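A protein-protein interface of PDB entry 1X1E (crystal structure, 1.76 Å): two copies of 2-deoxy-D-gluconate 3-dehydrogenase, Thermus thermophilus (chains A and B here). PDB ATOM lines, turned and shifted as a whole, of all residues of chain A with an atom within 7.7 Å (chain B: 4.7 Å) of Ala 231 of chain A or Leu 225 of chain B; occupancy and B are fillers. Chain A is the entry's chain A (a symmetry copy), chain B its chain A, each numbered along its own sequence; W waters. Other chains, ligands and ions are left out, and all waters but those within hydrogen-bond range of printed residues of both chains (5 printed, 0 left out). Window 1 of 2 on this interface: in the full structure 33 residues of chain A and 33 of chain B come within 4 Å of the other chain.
2 positions are printed for both chains.
Met 201 of chain A touches Tyr 224 of chain B.
Glu 223 of chain B touches Glu 209 of chain A.
CG of Leu 225 of chain B touches O of Ala 231 of chain A (3.5 Å).
CG of Gln 228 of chain B touches O of Ala 231 of chain A, at 3.4 Å.
Val 232 of chain A touches Tyr 224 of chain B.
OD1 of Asp 233 of chain A touches O of Thr 226 of chain B, 3.99 Å away.
Gly 234 of chain A touches Thr 226 of chain B (C to CG2, 3.6 Å).
Thr 226 of chain B touches Gly 235 of chain A (CG2 to N, 3.5 Å).
Leu 237 of chain A touches Gln 228 of chain B.
The guanidinium group of Arg 168 of chain B is in hydrogen-bond range of the side-chain sulfur of Met 201 of chain A.
N of Asp 233 of chain A lies within hydrogen-bond range of O of Tyr 224 of chain B, at 3.3 Å.
O of Tyr 224 of chain B lies within hydrogen-bond range of N of Gly 234 of chain A.
The backbone carbonyl oxygen (O) of Glu 223 of chain B lies close to the side-chain sulfur (SD) of Met 201 of chain A (3.4 Å).
Water W5 lies within hydrogen-bond range of OD1 of Asp 233 of chain A (2.7 Å), O of Ala 231 of chain A (2.8 Å) and N of Thr 226 of chain B (3.0 Å).
Water W3 bridges OE1 of Gln 228 of chain B (2.7 Å) and N of Ala 231 of chain A (3.1 Å).
Water W4 lies within hydrogen-bond range of the backbone carbonyl oxygen (O) of Asp 233 of chain A (2.7 Å) and the side-chain hydroxyl (OH) of Tyr 224 of chain B (2.9 Å).
Water W1 lies within hydrogen-bond range of OD1 of Asp 233 of chain A (2.8 Å), O of Thr 226 of chain B (2.9 Å) and NE2 of Gln 228 of chain B (3.0 Å).
Water W2 bridges the backbone carbonyl oxygen of Glu 209 of chain A and the backbone NH of Tyr 224 of chain B.
ND2 of Asn 170 of chain B lies within hydrogen-bond range of O of Leu 225 of chain B (2.9 Å).
The side-chain amide oxygen (OD1) of Asn 170 of chain B lies within hydrogen-bond range of the backbone NH (N) of Gln 228 of chain B, 3.1 Å away.
The backbone carbonyl oxygen of Val 232 of chain A is in hydrogen-bond range of the backbone NH of Gly 175 of chain A.
The backbone NH (N) of Met 201 of chain A sits at hydrogen-bond distance from the backbone carbonyl oxygen (O) of Gly 234 of chain A (3.3 Å).
N of Gly 235 of chain A sits at hydrogen-bond distance from OD1 of Asp 233 of chain A.
The side-chain carboxylate of Asp 233 of chain A is in hydrogen-bond range of the backbone NH of Leu 237 of chain A (2.8 Å).
Printed residues of chain B that touch a printed residue of chain A: Arg 168, Glu 223, Tyr 224, Leu 225, Thr 226 and Gln 228.
Hydrophobic or aromatic side chains of chain B within 4 Å of the printed part of chain A: Tyr 224 and Leu 225.
Of the 22 printed residues of chain A, 8 touch a printed residue of chain B.
Along chain A the printed residues that touch a printed residue of chain B span positions 201 to 237.
Ala 231 of chain A touches just these residues of chain B: Leu 225 (3.5 Å) and Gln 228 (3.4 Å).
Of the printed residues of chain B, Val 232 of chain A touches Tyr 224.
Of the printed residues of chain B, Leu 237 of chain A touches Gln 228.
Of the printed residues of chain A, Tyr 224 of chain B touches Met 201, Val 232, Asp 233 and Gly 234.
Printed residues of chain A within 4 Å of Gln 228 of chain B: Ala 231 and Leu 237.
Printed residues of chain A within 4 Å of Thr 226 of chain B: Asp 233 (3.99 Å), Gly 234 (3.6 Å) and Gly 235 (3.5 Å).
Val 213 of chain A touches none of the printed residues of chain B.
The nearest printed residue of chain B that does not touch Gly 235 of chain A is Tyr 224 of chain B (4.9 Å).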
ATOM      1  N   SER A 129      17.168  20.899 -11.740  1.00  0.00           N
ATOM      2  CA  SER A 129      18.256  20.616 -10.809  1.00  0.00           C
ATOM      3  C   SER A 129      18.462  21.838  -9.919  1.00  0.00           C
ATOM      4  O   SER A 129      17.803  22.864 -10.108  1.00  0.00           O
ATOM      5  CB  SER A 129      19.526  20.337 -11.623  1.00  0.00           C
ATOM      6  OG  SER A 129      20.705  20.480 -10.860  1.00  0.00           O
ATOM      7  N   VAL A 130      19.347  21.735  -8.930  1.00  0.00           N
ATOM      8  CA  VAL A 130      19.614  22.909  -8.113  1.00  0.00           C
ATOM      9  C   VAL A 130      20.376  23.845  -9.048  1.00  0.00           C
ATOM     10  O   VAL A 130      20.415  25.058  -8.828  1.00  0.00           O
ATOM     11  CB  VAL A 130      20.481  22.596  -6.858  1.00  0.00           C
ATOM     12  CG1 VAL A 130      19.722  21.674  -5.917  1.00  0.00           C
ATOM     13  CG2 VAL A 130      21.810  21.981  -7.263  1.00  0.00           C
ATOM     14  N   PHE A 133      19.104  27.007 -10.692  1.00  0.00           N
ATOM     15  CA  PHE A 133      19.209  28.253  -9.928  1.00  0.00           C
ATOM     16  C   PHE A 133      20.619  28.644  -9.474  1.00  0.00           C
ATOM     17  O   PHE A 133      20.834  29.772  -9.024  1.00  0.00           O
ATOM     18  CB  PHE A 133      18.303  28.152  -8.702  1.00  0.00           C
ATOM     19  CG  PHE A 133      16.870  27.866  -9.038  1.00  0.00           C
ATOM     20  CD1 PHE A 133      16.033  28.882  -9.486  1.00  0.00           C
ATOM     21  CD2 PHE A 133      16.364  26.573  -8.934  1.00  0.00           C
ATOM     22  CE1 PHE A 133      14.709  28.615  -9.828  1.00  0.00           C
ATOM     23  CE2 PHE A 133      15.043  26.295  -9.274  1.00  0.00           C
ATOM     24  CZ  PHE A 133      14.213  27.317  -9.721  1.00  0.00           C
ATOM     25  N   LEU A 171       8.525  22.198 -14.119  1.00  0.00           N
ATOM     26  CA  LEU A 171       9.900  21.721 -13.982  1.00  0.00           C
ATOM     27  C   LEU A 171      10.186  21.251 -12.554  1.00  0.00           C
ATOM     28  O   LEU A 171      10.221  22.057 -11.621  1.00  0.00           O
ATOM     29  CB  LEU A 171      10.873  22.850 -14.355  1.00  0.00           C
ATOM     30  CG  LEU A 171      12.385  22.605 -14.315  1.00  0.00           C
ATOM     31  CD1 LEU A 171      12.772  21.649 -15.445  1.00  0.00           C
ATOM     32  CD2 LEU A 171      13.125  23.928 -14.470  1.00  0.00           C
ATOM     33  N   LEU A 172      10.377  19.947 -12.387  1.00  0.00           N
ATOM     34  CA  LEU A 172      10.686  19.377 -11.077  1.00  0.00           C
ATOM     35  C   LEU A 172      12.191  19.480 -10.900  1.00  0.00           C
ATOM     36  O   LEU A 172      12.945  18.912 -11.684  1.00  0.00           O
ATOM     37  CB  LEU A 172      10.253  17.912 -11.019  1.00  0.00           C
ATOM     38  CG  LEU A 172      10.593  17.128  -9.748  1.00  0.00           C
ATOM     39  CD1 LEU A 172      10.057  17.838  -8.516  1.00  0.00           C
ATOM     40  CD2 LEU A 172       9.999  15.730  -9.864  1.00  0.00           C
ATOM     41  N   CYS A 173      12.623  20.203  -9.871  1.00  0.00           N
ATOM     42  CA  CYS A 173      14.044  20.399  -9.616  1.00  0.00           C
ATOM     43  C   CYS A 173      14.524  19.631  -8.398  1.00  0.00           C
ATOM     44  O   CYS A 173      14.450  20.115  -7.270  1.00  0.00           O
ATOM     45  CB  CYS A 173      14.343  21.885  -9.430  1.00  0.00           C
ATOM     46  SG  CYS A 173      14.038  22.863 -10.913  1.00  0.00           S
ATOM     47  N   PRO A 174      15.025  18.412  -8.615  1.00  0.00           N
ATOM     48  CA  PRO A 174      15.513  17.602  -7.496  1.00  0.00           C
ATOM     49  C   PRO A 174      16.819  18.162  -6.936  1.00  0.00           C
ATOM     50  O   PRO A 174      17.613  18.775  -7.659  1.00  0.00           O
ATOM     51  CB  PRO A 174      15.714  16.219  -8.122  1.00  0.00           C
ATOM     52  CG  PRO A 174      14.904  16.252  -9.396  1.00  0.00           C
ATOM     53  CD  PRO A 174      15.087  17.662  -9.878  1.00  0.00           C
ATOM     54  N   GLY A 175      17.038  17.965  -5.641  1.00  0.00           N
ATOM     55  CA  GLY A 175      18.276  18.420  -5.051  1.00  0.00           C
ATOM     56  C   GLY A 175      19.310  17.328  -5.255  1.00  0.00           C
ATOM     57  O   GLY A 175      19.424  16.768  -6.352  1.00  0.00           O
ATOM     58  N   MET A 201      18.420  19.581   5.909  1.00  0.00           N
ATOM     59  CA  MET A 201      17.994  18.263   6.363  1.00  0.00           C
ATOM     60  C   MET A 201      19.169  17.330   6.672  1.00  0.00           C
ATOM     61  O   MET A 201      18.988  16.260   7.254  1.00  0.00           O
ATOM     62  CB  MET A 201      17.038  17.637   5.341  1.00  0.00           C
ATOM     63  CG  MET A 201      15.622  18.217   5.438  1.00  0.00           C
ATOM     64  SD  MET A 201      14.428  17.483   4.298  1.00  0.00           S
ATOM     65  CE  MET A 201      14.511  15.756   4.801  1.00  0.00           C
ATOM     66  N   GLU A 209      11.522   9.747  -2.635  1.00  0.00           N
ATOM     67  CA  GLU A 209      11.070  10.993  -2.019  1.00  0.00           C
ATOM     68  C   GLU A 209      10.868  12.071  -3.080  1.00  0.00           C
ATOM     69  O   GLU A 209       9.979  12.909  -2.959  1.00  0.00           O
ATOM     70  CB  GLU A 209      12.068  11.460  -0.950  1.00  0.00           C
ATOM     71  CG  GLU A 209      12.146  10.505   0.244  1.00  0.00           C
ATOM     72  CD  GLU A 209      13.252  10.846   1.225  1.00  0.00           C
ATOM     73  OE1 GLU A 209      14.390  11.074   0.779  1.00  0.00           O
ATOM     74  OE2 GLU A 209      12.986  10.864   2.448  1.00  0.00           O
ATOM     75  N   ILE A 210      11.690  12.043  -4.122  1.00  0.00           N
ATOM     76  CA  ILE A 210      11.571  13.005  -5.217  1.00  0.00           C
ATOM     77  C   ILE A 210      10.332  12.654  -6.043  1.00  0.00           C
ATOM     78  O   ILE A 210       9.578  13.536  -6.464  1.00  0.00           O
ATOM     79  CB  ILE A 210      12.821  12.955  -6.142  1.00  0.00           C
ATOM     80  CG1 ILE A 210      14.094  13.218  -5.329  1.00  0.00           C
ATOM     81  CG2 ILE A 210      12.686  13.968  -7.266  1.00  0.00           C
ATOM     82  CD1 ILE A 210      14.146  14.568  -4.637  1.00  0.00           C
ATOM     83  N   VAL A 213       6.636  14.012  -5.280  1.00  0.00           N
ATOM     84  CA  VAL A 213       6.271  15.306  -5.848  1.00  0.00           C
ATOM     85  C   VAL A 213       6.047  15.201  -7.359  1.00  0.00           C
ATOM     86  O   VAL A 213       5.162  15.845  -7.908  1.00  0.00           O
ATOM     87  CB  VAL A 213       7.359  16.355  -5.540  1.00  0.00           C
ATOM     88  CG1 VAL A 213       6.915  17.734  -6.017  1.00  0.00           C
ATOM     89  CG2 VAL A 213       7.634  16.369  -4.044  1.00  0.00           C
ATOM     90  N   LEU A 217       2.788  16.503  -9.692  1.00  0.00           N
ATOM     91  CA  LEU A 217       2.873  17.351 -10.873  1.00  0.00           C
ATOM     92  C   LEU A 217       2.401  16.642 -12.131  1.00  0.00           C
ATOM     93  O   LEU A 217       2.312  17.253 -13.191  1.00  0.00           O
ATOM     94  CB  LEU A 217       4.307  17.861 -11.045  1.00  0.00           C
ATOM     95  CG  LEU A 217       4.792  18.738  -9.881  1.00  0.00           C
ATOM     96  CD1 LEU A 217       6.279  19.029 -10.045  1.00  0.00           C
ATOM     97  CD2 LEU A 217       4.002  20.048  -9.840  1.00  0.00           C
ATOM     98  N   GLN A 228       5.748  26.543 -13.755  1.00  0.00           N
ATOM     99  CA  GLN A 228       6.565  26.726 -12.557  1.00  0.00           C
ATOM    100  C   GLN A 228       7.631  25.671 -12.327  1.00  0.00           C
ATOM    101  O   GLN A 228       7.552  24.559 -12.837  1.00  0.00           O
ATOM    102  CB  GLN A 228       5.672  26.748 -11.307  1.00  0.00           C
ATOM    103  CG  GLN A 228       4.839  28.009 -11.131  1.00  0.00           C
ATOM    104  CD  GLN A 228       5.706  29.231 -10.952  1.00  0.00           C
ATOM    105  OE1 GLN A 228       6.604  29.248 -10.111  1.00  0.00           O
ATOM    106  NE2 GLN A 228       5.447  30.266 -11.743  1.00  0.00           N
ATOM    107  N   ALA A 229       8.629  26.040 -11.537  1.00  0.00           N
ATOM    108  CA  ALA A 229       9.685  25.109 -11.170  1.00  0.00           C
ATOM    109  C   ALA A 229       9.384  24.774  -9.713  1.00  0.00           C
ATOM    110  O   ALA A 229       8.971  25.646  -8.949  1.00  0.00           O
ATOM    111  CB  ALA A 229      11.056  25.772 -11.280  1.00  0.00           C
ATOM    112  N   VAL A 230       9.559  23.516  -9.335  1.00  0.00           N
ATOM    113  CA  VAL A 230       9.331  23.113  -7.951  1.00  0.00           C
ATOM    114  C   VAL A 230      10.588  22.401  -7.474  1.00  0.00           C
ATOM    115  O   VAL A 230      10.930  21.326  -7.966  1.00  0.00           O
ATOM    116  CB  VAL A 230       8.111  22.175  -7.823  1.00  0.00           C
ATOM    117  CG1 VAL A 230       7.933  21.751  -6.373  1.00  0.00           C
ATOM    118  CG2 VAL A 230       6.856  22.891  -8.319  1.00  0.00           C
ATOM    119  N   ALA A 231      11.281  23.018  -6.521  1.00  0.00           N
ATOM    120  CA  ALA A 231      12.518  22.460  -5.991  1.00  0.00           C
ATOM    121  C   ALA A 231      12.266  21.580  -4.777  1.00  0.00           C
ATOM    122  O   ALA A 231      11.644  22.004  -3.800  1.00  0.00           O
ATOM    123  CB  ALA A 231      13.484  23.589  -5.628  1.00  0.00           C
ATOM    124  N   VAL A 232      12.757  20.348  -4.856  1.00  0.00           N
ATOM    125  CA  VAL A 232      12.627  19.360  -3.786  1.00  0.00           C
ATOM    126  C   VAL A 232      14.087  19.063  -3.467  1.00  0.00           C
ATOM    127  O   VAL A 232      14.675  18.121  -4.008  1.00  0.00           O
ATOM    128  CB  VAL A 232      11.910  18.092  -4.307  1.00  0.00           C
ATOM    129  CG1 VAL A 232      11.626  17.134  -3.163  1.00  0.00           C
ATOM    130  CG2 VAL A 232      10.604  18.491  -4.993  1.00  0.00           C
ATOM    131  N   ASP A 233      14.667  19.870  -2.583  1.00  0.00           N
ATOM    132  CA  ASP A 233      16.091  19.760  -2.279  1.00  0.00           C
ATOM    133  C   ASP A 233      16.520  19.698  -0.824  1.00  0.00           C
ATOM    134  O   ASP A 233      17.687  19.968  -0.513  1.00  0.00           O
ATOM    135  CB  ASP A 233      16.818  20.933  -2.941  1.00  0.00           C
ATOM    136  CG  ASP A 233      16.409  22.277  -2.357  1.00  0.00           C
ATOM    137  OD1 ASP A 233      15.539  22.303  -1.460  1.00  0.00           O
ATOM    138  OD2 ASP A 233      16.960  23.307  -2.791  1.00  0.00           O
ATOM    139  N   GLY A 234      15.595  19.364   0.067  1.00  0.00           N
ATOM    140  CA  GLY A 234      15.948  19.276   1.472  1.00  0.00           C
ATOM    141  C   GLY A 234      16.392  20.597   2.073  1.00  0.00           C
ATOM    142  O   GLY A 234      16.995  20.619   3.147  1.00  0.00           O
ATOM    143  N   GLY A 235      16.096  21.692   1.377  1.00  0.00           N
ATOM    144  CA  GLY A 235      16.451  23.013   1.863  1.00  0.00           C
ATOM    145  C   GLY A 235      17.746  23.605   1.345  1.00  0.00           C
ATOM    146  O   GLY A 235      18.121  24.707   1.740  1.00  0.00           O
ATOM    147  N   LEU A 237      18.735  25.104  -1.499  1.00  0.00           N
ATOM    148  CA  LEU A 237      18.654  26.437  -2.083  1.00  0.00           C
ATOM    149  C   LEU A 237      18.300  27.531  -1.076  1.00  0.00           C
ATOM    150  O   LEU A 237      18.736  28.677  -1.214  1.00  0.00           O
ATOM    151  CB  LEU A 237      17.648  26.436  -3.245  1.00  0.00           C
ATOM    152  CG  LEU A 237      18.080  25.604  -4.463  1.00  0.00           C
ATOM    153  CD1 LEU A 237      16.980  25.574  -5.516  1.00  0.00           C
ATOM    154  CD2 LEU A 237      19.348  26.200  -5.046  1.00  0.00           C
ATOM    155  N   ARG B 168       9.097  20.851   8.014  1.00  0.00           N
ATOM    156  CA  ARG B 168       9.279  21.363   6.658  1.00  0.00           C
ATOM    157  C   ARG B 168       8.456  22.644   6.627  1.00  0.00           C
ATOM    158  O   ARG B 168       7.338  22.681   7.142  1.00  0.00           O
ATOM    159  CB  ARG B 168       8.750  20.380   5.609  1.00  0.00           C
ATOM    160  CG  ARG B 168       9.283  18.971   5.756  1.00  0.00           C
ATOM    161  CD  ARG B 168      10.798  18.916   5.635  1.00  0.00           C
ATOM    162  NE  ARG B 168      11.315  17.596   5.992  1.00  0.00           N
ATOM    163  CZ  ARG B 168      12.061  17.357   7.066  1.00  0.00           C
ATOM    164  NH1 ARG B 168      12.375  18.346   7.889  1.00  0.00           N
ATOM    165  NH2 ARG B 168      12.497  16.127   7.310  1.00  0.00           N
ATOM    166  N   ASN B 170       7.193  25.800   4.007  1.00  0.00           N
ATOM    167  CA  ASN B 170       7.061  26.277   2.634  1.00  0.00           C
ATOM    168  C   ASN B 170       6.022  27.388   2.498  1.00  0.00           C
ATOM    169  O   ASN B 170       5.228  27.628   3.410  1.00  0.00           O
ATOM    170  CB  ASN B 170       6.695  25.099   1.731  1.00  0.00           C
ATOM    171  CG  ASN B 170       7.780  24.039   1.700  1.00  0.00           C
ATOM    172  OD1 ASN B 170       8.879  24.286   1.205  1.00  0.00           O
ATOM    173  ND2 ASN B 170       7.481  22.863   2.231  1.00  0.00           N
ATOM    174  N   LEU B 217       1.650  19.987   0.491  1.00  0.00           N
ATOM    175  CA  LEU B 217       2.678  20.652   1.278  1.00  0.00           C
ATOM    176  C   LEU B 217       2.484  20.454   2.772  1.00  0.00           C
ATOM    177  O   LEU B 217       3.323  20.864   3.567  1.00  0.00           O
ATOM    178  CB  LEU B 217       2.716  22.143   0.931  1.00  0.00           C
ATOM    179  CG  LEU B 217       3.083  22.424  -0.534  1.00  0.00           C
ATOM    180  CD1 LEU B 217       2.902  23.908  -0.832  1.00  0.00           C
ATOM    181  CD2 LEU B 217       4.530  22.006  -0.808  1.00  0.00           C
ATOM    182  N   ALA B 222       5.809  16.216   0.941  1.00  0.00           N
ATOM    183  CA  ALA B 222       6.800  17.271   1.149  1.00  0.00           C
ATOM    184  C   ALA B 222       7.971  16.867   2.050  1.00  0.00           C
ATOM    185  O   ALA B 222       8.718  17.718   2.523  1.00  0.00           O
ATOM    186  CB  ALA B 222       6.116  18.506   1.719  1.00  0.00           C
ATOM    187  N   GLU B 223       8.146  15.574   2.283  1.00  0.00           N
ATOM    188  CA  GLU B 223       9.237  15.114   3.138  1.00  0.00           C
ATOM    189  C   GLU B 223      10.592  15.752   2.811  1.00  0.00           C
ATOM    190  O   GLU B 223      11.339  16.113   3.719  1.00  0.00           O
ATOM    191  CB  GLU B 223       9.345  13.588   3.065  1.00  0.00           C
ATOM    192  CG  GLU B 223      10.499  12.997   3.862  1.00  0.00           C
ATOM    193  CD  GLU B 223      10.544  13.520   5.282  1.00  0.00           C
ATOM    194  OE1 GLU B 223       9.481  13.543   5.938  1.00  0.00           O
ATOM    195  OE2 GLU B 223      11.642  13.901   5.741  1.00  0.00           O
ATOM    196  N   TYR B 224      10.908  15.903   1.527  1.00  0.00           N
ATOM    197  CA  TYR B 224      12.186  16.496   1.126  1.00  0.00           C
ATOM    198  C   TYR B 224      11.983  17.858   0.441  1.00  0.00           C
ATOM    199  O   TYR B 224      12.859  18.346  -0.273  1.00  0.00           O
ATOM    200  CB  TYR B 224      12.936  15.541   0.182  1.00  0.00           C
ATOM    201  CG  TYR B 224      14.446  15.705   0.190  1.00  0.00           C
ATOM    202  CD1 TYR B 224      15.215  15.226   1.253  1.00  0.00           C
ATOM    203  CD2 TYR B 224      15.102  16.344  -0.860  1.00  0.00           C
ATOM    204  CE1 TYR B 224      16.607  15.381   1.271  1.00  0.00           C
ATOM    205  CE2 TYR B 224      16.492  16.508  -0.853  1.00  0.00           C
ATOM    206  CZ  TYR B 224      17.236  16.025   0.216  1.00  0.00           C
ATOM    207  OH  TYR B 224      18.605  16.195   0.227  1.00  0.00           O
ATOM    208  N   LEU B 225      10.827  18.473   0.669  1.00  0.00           N
ATOM    209  CA  LEU B 225      10.524  19.767   0.068  1.00  0.00           C
ATOM    210  C   LEU B 225      10.395  20.796   1.183  1.00  0.00           C
ATOM    211  O   LEU B 225       9.428  20.775   1.945  1.00  0.00           O
ATOM    212  CB  LEU B 225       9.214  19.681  -0.730  1.00  0.00           C
ATOM    213  CG  LEU B 225       9.010  20.685  -1.871  1.00  0.00           C
ATOM    214  CD1 LEU B 225       7.731  20.338  -2.620  1.00  0.00           C
ATOM    215  CD2 LEU B 225       8.947  22.104  -1.327  1.00  0.00           C
ATOM    216  N   THR B 226      11.367  21.695   1.285  1.00  0.00           N
ATOM    217  CA  THR B 226      11.325  22.703   2.340  1.00  0.00           C
ATOM    218  C   THR B 226      12.082  23.983   1.963  1.00  0.00           C
ATOM    219  O   THR B 226      13.043  23.946   1.189  1.00  0.00           O
ATOM    220  CB  THR B 226      11.891  22.117   3.656  1.00  0.00           C
ATOM    221  OG1 THR B 226      11.598  22.995   4.748  1.00  0.00           O
ATOM    222  CG2 THR B 226      13.403  21.922   3.548  1.00  0.00           C
ATOM    223  N   GLY B 227      11.633  25.106   2.516  1.00  0.00           N
ATOM    224  CA  GLY B 227      12.248  26.395   2.239  1.00  0.00           C
ATOM    225  C   GLY B 227      11.929  26.919   0.850  1.00  0.00           C
ATOM    226  O   GLY B 227      12.658  27.756   0.318  1.00  0.00           O
ATOM    227  N   GLN B 228      10.830  26.448   0.266  1.00  0.00           N
ATOM    228  CA  GLN B 228      10.446  26.853  -1.085  1.00  0.00           C
ATOM    229  C   GLN B 228       9.077  27.497  -1.208  1.00  0.00           C
ATOM    230  O   GLN B 228       8.207  27.319  -0.364  1.00  0.00           O
ATOM    231  CB  GLN B 228      10.460  25.638  -2.025  1.00  0.00           C
ATOM    232  CG  GLN B 228      11.845  25.125  -2.396  1.00  0.00           C
ATOM    233  CD  GLN B 228      12.636  26.158  -3.161  1.00  0.00           C
ATOM    234  OE1 GLN B 228      12.158  26.711  -4.150  1.00  0.00           O
ATOM    235  NE2 GLN B 228      13.855  26.427  -2.709  1.00  0.00           N
HETATM  236  O   HOH W   1      15.157  24.915  -0.482  1.00  0.00           O
HETATM  237  O   HOH W   2       9.547  14.830  -0.895  1.00  0.00           O
HETATM  238  O   HOH W   3      10.130  25.736  -5.631  1.00  0.00           O
HETATM  239  O   HOH W   4      19.432  18.215  -1.700  1.00  0.00           O
HETATM  240  O   HOH W   5      12.916  21.746  -1.294  1.00  0.00           O
